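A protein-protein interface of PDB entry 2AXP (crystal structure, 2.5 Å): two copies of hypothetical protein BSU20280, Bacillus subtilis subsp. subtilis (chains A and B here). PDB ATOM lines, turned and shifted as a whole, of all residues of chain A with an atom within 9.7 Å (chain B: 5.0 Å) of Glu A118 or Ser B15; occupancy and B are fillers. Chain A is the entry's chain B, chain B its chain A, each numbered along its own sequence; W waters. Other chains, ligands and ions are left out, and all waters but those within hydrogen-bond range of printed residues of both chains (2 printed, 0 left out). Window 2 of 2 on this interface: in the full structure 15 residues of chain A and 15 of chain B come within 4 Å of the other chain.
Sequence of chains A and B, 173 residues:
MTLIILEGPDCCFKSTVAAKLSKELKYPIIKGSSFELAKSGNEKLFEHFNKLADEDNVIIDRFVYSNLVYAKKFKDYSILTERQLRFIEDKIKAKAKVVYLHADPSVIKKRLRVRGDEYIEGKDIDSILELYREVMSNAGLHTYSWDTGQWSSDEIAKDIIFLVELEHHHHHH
N of Glu A118 is in hydrogen-bond range of OD2 of Asp B10.
The backbone carbonyl oxygen (O) of Glu A118 sits at hydrogen-bond distance from the guanidinium group (NH1) of Arg B62 (3.3 Å).
Among the printed residues, merely in contact across the chains: Glu A118 with Lys B14 (3.3 Å), Glu A118 with Ser B15 (3.5 Å), Tyr A119 with Asp B10 (3.4 Å) and Tyr A119 with Arg B62 (3.8 Å).
Arg A113 touches none of the printed residues of chain B.
Of chain B, only Asp B10 (3.5 Å), Lys B14 (3.3 Å), Ser B15 (3.5 Å) and Arg B62 (3.3 Å) come within 4 Å of Glu A118.
Printed residues of chain B within 4 Å of Tyr A119: Asp B10 and Arg B62.
Of the printed residues of chain A, Asp B10 touches Glu A118 (3.5 Å) and Tyr A119 (3.4 Å).
Ser B15 touches just one residue of chain A: Glu A118 (3.5 Å).
No residue of chain A comes within 4 Å of Thr B16.
Ala B18 touches none of the printed residues of chain A.
Printed residues of chain A within 4 Å of Arg B62: Glu A118 and Tyr A119.
The nearest residue of chain B that does not touch Glu A118 is Phe B13 (4.7 Å).
The nearest residue of chain A that does not touch Ser B15 is Gly A116 (6.6 Å).
Of the 12 printed residues of chain B, 4 touch a printed residue of chain A.
Water W2 lies within hydrogen-bond range of N of Cys B11 (2.5 Å), OE2 of Glu A118 (3.2 Å) and OD2 of Asp B10 (3.3 Å).
Water W1 bridges N of Phe B13 (2.7 Å) and OE2 of Glu A118 (3.1 Å).
The backbone carbonyl oxygen of Pro B9 lies within hydrogen-bond range of the side-chain amino group of Lys B14 (3.4 Å).
NH2 of Arg B62 lies within salt-bridge range of OD2 of Asp B61 (3.6 Å).
OH of Tyr A119 sits close to OD1 of Asp A117, at 3.3 Å.
No position is printed for both chains.
Of the 6 pairs that touch across the chains among the printed residues, none has its exchanged pair printed and touching as well.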
ATOM      1  N   LEU A 112     -12.507  16.548  20.802  1.00  0.00           N
ATOM      2  CA  LEU A 112     -13.672  16.737  19.956  1.00  0.00           C
ATOM      3  C   LEU A 112     -14.606  15.564  20.190  1.00  0.00           C
ATOM      4  O   LEU A 112     -15.812  15.740  20.363  1.00  0.00           O
ATOM      5  CB  LEU A 112     -13.246  16.807  18.484  1.00  0.00           C
ATOM      6  CG  LEU A 112     -12.761  18.163  17.968  1.00  0.00           C
ATOM      7  CD1 LEU A 112     -12.053  18.012  16.638  1.00  0.00           C
ATOM      8  CD2 LEU A 112     -13.950  19.088  17.827  1.00  0.00           C
ATOM      9  N   ARG A 113     -14.044  14.360  20.201  1.00  0.00           N
ATOM     10  CA  ARG A 113     -14.860  13.180  20.438  1.00  0.00           C
ATOM     11  C   ARG A 113     -15.499  13.279  21.812  1.00  0.00           C
ATOM     12  O   ARG A 113     -16.691  12.999  21.981  1.00  0.00           O
ATOM     13  CB  ARG A 113     -14.022  11.908  20.327  1.00  0.00           C
ATOM     14  CG  ARG A 113     -13.834  11.464  18.874  1.00  0.00           C
ATOM     15  CD  ARG A 113     -13.101  10.140  18.781  1.00  0.00           C
ATOM     16  NE  ARG A 113     -11.682  10.328  18.501  1.00  0.00           N
ATOM     17  CZ  ARG A 113     -11.196  10.632  17.302  1.00  0.00           C
ATOM     18  NH1 ARG A 113      -9.885  10.787  17.140  1.00  0.00           N
ATOM     19  NH2 ARG A 113     -12.019  10.764  16.263  1.00  0.00           N
ATOM     20  N   VAL A 114     -14.707  13.702  22.788  1.00  0.00           N
ATOM     21  CA  VAL A 114     -15.214  13.851  24.135  1.00  0.00           C
ATOM     22  C   VAL A 114     -16.383  14.828  24.205  1.00  0.00           C
ATOM     23  O   VAL A 114     -17.287  14.662  25.021  1.00  0.00           O
ATOM     24  CB  VAL A 114     -14.122  14.335  25.065  1.00  0.00           C
ATOM     25  CG1 VAL A 114     -14.703  14.595  26.435  1.00  0.00           C
ATOM     26  CG2 VAL A 114     -13.027  13.299  25.137  1.00  0.00           C
ATOM     27  N   ARG A 115     -16.367  15.840  23.345  1.00  0.00           N
ATOM     28  CA  ARG A 115     -17.429  16.836  23.332  1.00  0.00           C
ATOM     29  C   ARG A 115     -18.658  16.336  22.576  1.00  0.00           C
ATOM     30  O   ARG A 115     -19.768  16.822  22.793  1.00  0.00           O
ATOM     31  CB  ARG A 115     -16.914  18.138  22.719  1.00  0.00           C
ATOM     32  CG  ARG A 115     -17.774  19.338  23.043  1.00  0.00           C
ATOM     33  CD  ARG A 115     -16.949  20.603  23.066  1.00  0.00           C
ATOM     34  NE  ARG A 115     -16.480  20.996  21.738  1.00  0.00           N
ATOM     35  CZ  ARG A 115     -15.742  22.077  21.515  1.00  0.00           C
ATOM     36  NH1 ARG A 115     -15.353  22.378  20.283  1.00  0.00           N
ATOM     37  NH2 ARG A 115     -15.388  22.855  22.534  1.00  0.00           N
ATOM     38  N   GLY A 116     -18.455  15.374  21.679  1.00  0.00           N
ATOM     39  CA  GLY A 116     -19.575  14.806  20.952  1.00  0.00           C
ATOM     40  C   GLY A 116     -19.914  15.308  19.564  1.00  0.00           C
ATOM     41  O   GLY A 116     -21.094  15.408  19.220  1.00  0.00           O
ATOM     42  N   ASP A 117     -18.905  15.616  18.757  1.00  0.00           N
ATOM     43  CA  ASP A 117     -19.152  16.094  17.397  1.00  0.00           C
ATOM     44  C   ASP A 117     -19.611  14.964  16.482  1.00  0.00           C
ATOM     45  O   ASP A 117     -19.249  13.804  16.682  1.00  0.00           O
ATOM     46  CB  ASP A 117     -17.889  16.718  16.810  1.00  0.00           C
ATOM     47  CG  ASP A 117     -17.696  18.156  17.233  1.00  0.00           C
ATOM     48  OD1 ASP A 117     -16.748  18.786  16.725  1.00  0.00           O
ATOM     49  OD2 ASP A 117     -18.479  18.665  18.065  1.00  0.00           O
ATOM     50  N   GLU A 118     -20.406  15.310  15.474  1.00  0.00           N
ATOM     51  CA  GLU A 118     -20.902  14.324  14.516  1.00  0.00           C
ATOM     52  C   GLU A 118     -20.343  14.568  13.114  1.00  0.00           C
ATOM     53  O   GLU A 118     -20.279  13.655  12.289  1.00  0.00           O
ATOM     54  CB  GLU A 118     -22.434  14.347  14.480  1.00  0.00           C
ATOM     55  CG  GLU A 118     -23.084  13.342  15.423  1.00  0.00           C
ATOM     56  CD  GLU A 118     -24.605  13.439  15.450  1.00  0.00           C
ATOM     57  OE1 GLU A 118     -25.215  13.625  14.365  1.00  0.00           O
ATOM     58  OE2 GLU A 118     -25.187  13.309  16.556  1.00  0.00           O
ATOM     59  N   TYR A 119     -19.938  15.810  12.860  1.00  0.00           N
ATOM     60  CA  TYR A 119     -19.377  16.215  11.569  1.00  0.00           C
ATOM     61  C   TYR A 119     -17.855  16.058  11.602  1.00  0.00           C
ATOM     62  O   TYR A 119     -17.182  16.238  10.587  1.00  0.00           O
ATOM     63  CB  TYR A 119     -19.729  17.685  11.274  1.00  0.00           C
ATOM     64  CG  TYR A 119     -19.010  18.687  12.169  1.00  0.00           C
ATOM     65  CD1 TYR A 119     -19.324  18.798  13.533  1.00  0.00           C
ATOM     66  CD2 TYR A 119     -17.980  19.494  11.659  1.00  0.00           C
ATOM     67  CE1 TYR A 119     -18.625  19.685  14.372  1.00  0.00           C
ATOM     68  CE2 TYR A 119     -17.277  20.380  12.486  1.00  0.00           C
ATOM     69  CZ  TYR A 119     -17.602  20.471  13.841  1.00  0.00           C
ATOM     70  OH  TYR A 119     -16.893  21.329  14.655  1.00  0.00           O
ATOM     71  N   ILE A 120     -17.334  15.735  12.786  1.00  0.00           N
ATOM     72  CA  ILE A 120     -15.900  15.552  13.010  1.00  0.00           C
ATOM     73  C   ILE A 120     -15.254  14.836  11.831  1.00  0.00           C
ATOM     74  O   ILE A 120     -15.358  13.615  11.698  1.00  0.00           O
ATOM     75  CB  ILE A 120     -15.652  14.763  14.350  1.00  0.00           C
ATOM     76  CG1 ILE A 120     -14.152  14.493  14.564  1.00  0.00           C
ATOM     77  CG2 ILE A 120     -16.499  13.490  14.370  1.00  0.00           C
ATOM     78  CD1 ILE A 120     -13.609  13.211  13.937  1.00  0.00           C
ATOM     79  N   GLU A 121     -14.605  15.603  10.958  1.00  0.00           N
ATOM     80  CA  GLU A 121     -13.960  15.013   9.788  1.00  0.00           C
ATOM     81  C   GLU A 121     -13.062  13.841  10.195  1.00  0.00           C
ATOM     82  O   GLU A 121     -13.440  12.672  10.037  1.00  0.00           O
ATOM     83  CB  GLU A 121     -13.133  16.064   9.038  1.00  0.00           C
ATOM     84  CG  GLU A 121     -13.945  17.096   8.264  1.00  0.00           C
ATOM     85  CD  GLU A 121     -14.690  18.079   9.154  1.00  0.00           C
ATOM     86  OE1 GLU A 121     -14.061  18.672  10.061  1.00  0.00           O
ATOM     87  OE2 GLU A 121     -15.905  18.276   8.935  1.00  0.00           O
ATOM     88  N   GLY A 122     -11.883  14.172  10.727  1.00  0.00           N
ATOM     89  CA  GLY A 122     -10.920  13.168  11.159  1.00  0.00           C
ATOM     90  C   GLY A 122      -9.508  13.451  10.661  1.00  0.00           C
ATOM     91  O   GLY A 122      -8.544  12.832  11.112  1.00  0.00           O
ATOM     92  N   PRO B   9     -29.220  18.151  10.936  1.00  0.00           N
ATOM     93  CA  PRO B   9     -28.140  18.858  11.624  1.00  0.00           C
ATOM     94  C   PRO B   9     -27.701  18.177  12.883  1.00  0.00           C
ATOM     95  O   PRO B   9     -28.348  17.238  13.342  1.00  0.00           O
ATOM     96  CB  PRO B   9     -28.740  20.226  11.879  1.00  0.00           C
ATOM     97  CG  PRO B   9     -30.164  19.899  12.164  1.00  0.00           C
ATOM     98  CD  PRO B   9     -30.507  18.846  11.129  1.00  0.00           C
ATOM     99  N   ASP B  10     -26.575  18.634  13.417  1.00  0.00           N
ATOM    100  CA  ASP B  10     -26.010  18.099  14.653  1.00  0.00           C
ATOM    101  C   ASP B  10     -26.933  18.399  15.823  1.00  0.00           C
ATOM    102  O   ASP B  10     -27.953  19.082  15.683  1.00  0.00           O
ATOM    103  CB  ASP B  10     -24.659  18.762  14.935  1.00  0.00           C
ATOM    104  CG  ASP B  10     -23.559  18.232  14.057  1.00  0.00           C
ATOM    105  OD1 ASP B  10     -23.812  18.056  12.843  1.00  0.00           O
ATOM    106  OD2 ASP B  10     -22.437  18.006  14.581  1.00  0.00           O
ATOM    107  N   CYS B  11     -26.556  17.884  16.980  1.00  0.00           N
ATOM    108  CA  CYS B  11     -27.310  18.129  18.186  1.00  0.00           C
ATOM    109  C   CYS B  11     -28.771  17.731  18.096  1.00  0.00           C
ATOM    110  O   CYS B  11     -29.628  18.313  18.774  1.00  0.00           O
ATOM    111  CB  CYS B  11     -27.209  19.605  18.566  1.00  0.00           C
ATOM    112  SG  CYS B  11     -25.533  20.063  19.057  1.00  0.00           S
ATOM    113  N   PHE B  13     -29.517  14.296  18.168  1.00  0.00           N
ATOM    114  CA  PHE B  13     -29.519  12.886  18.587  1.00  0.00           C
ATOM    115  C   PHE B  13     -29.582  11.851  17.458  1.00  0.00           C
ATOM    116  O   PHE B  13     -30.092  10.742  17.643  1.00  0.00           O
ATOM    117  CB  PHE B  13     -30.700  12.647  19.523  1.00  0.00           C
ATOM    118  CG  PHE B  13     -30.828  13.675  20.590  1.00  0.00           C
ATOM    119  CD1 PHE B  13     -29.910  13.726  21.627  1.00  0.00           C
ATOM    120  CD2 PHE B  13     -31.857  14.611  20.544  1.00  0.00           C
ATOM    121  CE1 PHE B  13     -30.011  14.696  22.610  1.00  0.00           C
ATOM    122  CE2 PHE B  13     -31.972  15.587  21.516  1.00  0.00           C
ATOM    123  CZ  PHE B  13     -31.046  15.634  22.558  1.00  0.00           C
ATOM    124  N   LYS B  14     -29.059  12.218  16.297  1.00  0.00           N
ATOM    125  CA  LYS B  14     -29.048  11.334  15.152  1.00  0.00           C
ATOM    126  C   LYS B  14     -28.263  10.070  15.512  1.00  0.00           C
ATOM    127  O   LYS B  14     -28.718   8.958  15.284  1.00  0.00           O
ATOM    128  CB  LYS B  14     -28.381  12.038  13.981  1.00  0.00           C
ATOM    129  CG  LYS B  14     -28.923  11.705  12.611  1.00  0.00           C
ATOM    130  CD  LYS B  14     -27.828  11.914  11.561  1.00  0.00           C
ATOM    131  CE  LYS B  14     -27.116  13.238  11.757  1.00  0.00           C
ATOM    132  NZ  LYS B  14     -28.111  14.337  11.607  1.00  0.00           N
ATOM    133  N   SER B  15     -27.087  10.242  16.089  1.00  0.00           N
ATOM    134  CA  SER B  15     -26.280   9.101  16.451  1.00  0.00           C
ATOM    135  C   SER B  15     -26.927   8.270  17.549  1.00  0.00           C
ATOM    136  O   SER B  15     -26.658   7.072  17.669  1.00  0.00           O
ATOM    137  CB  SER B  15     -24.905   9.548  16.922  1.00  0.00           C
ATOM    138  OG  SER B  15     -25.015  10.193  18.175  1.00  0.00           O
ATOM    139  N   THR B  16     -27.765   8.885  18.370  1.00  0.00           N
ATOM    140  CA  THR B  16     -28.401   8.119  19.433  1.00  0.00           C
ATOM    141  C   THR B  16     -29.587   7.353  18.868  1.00  0.00           C
ATOM    142  O   THR B  16     -29.818   6.206  19.226  1.00  0.00           O
ATOM    143  CB  THR B  16     -28.860   9.028  20.612  1.00  0.00           C
ATOM    144  OG1 THR B  16     -27.708   9.481  21.330  1.00  0.00           O
ATOM    145  CG2 THR B  16     -29.749   8.252  21.576  1.00  0.00           C
ATOM    146  N   VAL B  17     -30.337   7.988  17.979  1.00  0.00           N
ATOM    147  CA  VAL B  17     -31.475   7.333  17.370  1.00  0.00           C
ATOM    148  C   VAL B  17     -31.004   6.166  16.520  1.00  0.00           C
ATOM    149  O   VAL B  17     -31.701   5.151  16.378  1.00  0.00           O
ATOM    150  CB  VAL B  17     -32.240   8.300  16.501  1.00  0.00           C
ATOM    151  CG1 VAL B  17     -33.232   7.556  15.636  1.00  0.00           C
ATOM    152  CG2 VAL B  17     -32.948   9.297  17.389  1.00  0.00           C
ATOM    153  N   ALA B  18     -29.806   6.304  15.966  1.00  0.00           N
ATOM    154  CA  ALA B  18     -29.240   5.255  15.130  1.00  0.00           C
ATOM    155  C   ALA B  18     -28.870   4.051  15.991  1.00  0.00           C
ATOM    156  O   ALA B  18     -29.158   2.903  15.633  1.00  0.00           O
ATOM    157  CB  ALA B  18     -28.009   5.779  14.389  1.00  0.00           C
ATOM    158  N   ALA B  19     -28.242   4.322  17.133  1.00  0.00           N
ATOM    159  CA  ALA B  19     -27.828   3.260  18.049  1.00  0.00           C
ATOM    160  C   ALA B  19     -29.013   2.363  18.434  1.00  0.00           C
ATOM    161  O   ALA B  19     -28.920   1.136  18.396  1.00  0.00           O
ATOM    162  CB  ALA B  19     -27.208   3.876  19.297  1.00  0.00           C
ATOM    163  N   ASP B  61     -26.087   6.983   8.442  1.00  0.00           N
ATOM    164  CA  ASP B  61     -26.069   8.248   9.146  1.00  0.00           C
ATOM    165  C   ASP B  61     -25.519   9.252   8.125  1.00  0.00           C
ATOM    166  O   ASP B  61     -24.318   9.270   7.835  1.00  0.00           O
ATOM    167  CB  ASP B  61     -25.165   8.093  10.371  1.00  0.00           C
ATOM    168  CG  ASP B  61     -24.961   9.382  11.126  1.00  0.00           C
ATOM    169  OD1 ASP B  61     -24.356   9.301  12.222  1.00  0.00           O
ATOM    170  OD2 ASP B  61     -25.389  10.466  10.635  1.00  0.00           O
ATOM    171  N   ARG B  62     -26.435  10.048   7.568  1.00  0.00           N
ATOM    172  CA  ARG B  62     -26.167  11.074   6.543  1.00  0.00           C
ATOM    173  C   ARG B  62     -25.907  10.474   5.139  1.00  0.00           C
ATOM    174  O   ARG B  62     -25.038   9.617   4.946  1.00  0.00           O
ATOM    175  CB  ARG B  62     -25.023  11.999   6.995  1.00  0.00           C
ATOM    176  CG  ARG B  62     -25.389  12.773   8.263  1.00  0.00           C
ATOM    177  CD  ARG B  62     -24.924  14.225   8.248  1.00  0.00           C
ATOM    178  NE  ARG B  62     -23.470  14.308   8.259  1.00  0.00           N
ATOM    179  CZ  ARG B  62     -22.712  13.897   9.269  1.00  0.00           C
ATOM    180  NH1 ARG B  62     -21.387  14.002   9.186  1.00  0.00           N
ATOM    181  NH2 ARG B  62     -23.281  13.399  10.367  1.00  0.00           N
HETATM  182  O   HOH W   1     -26.930  14.577  18.798  1.00  0.00           O
HETATM  183  O   HOH W   2     -24.527  16.469  16.547  1.00  0.00           O
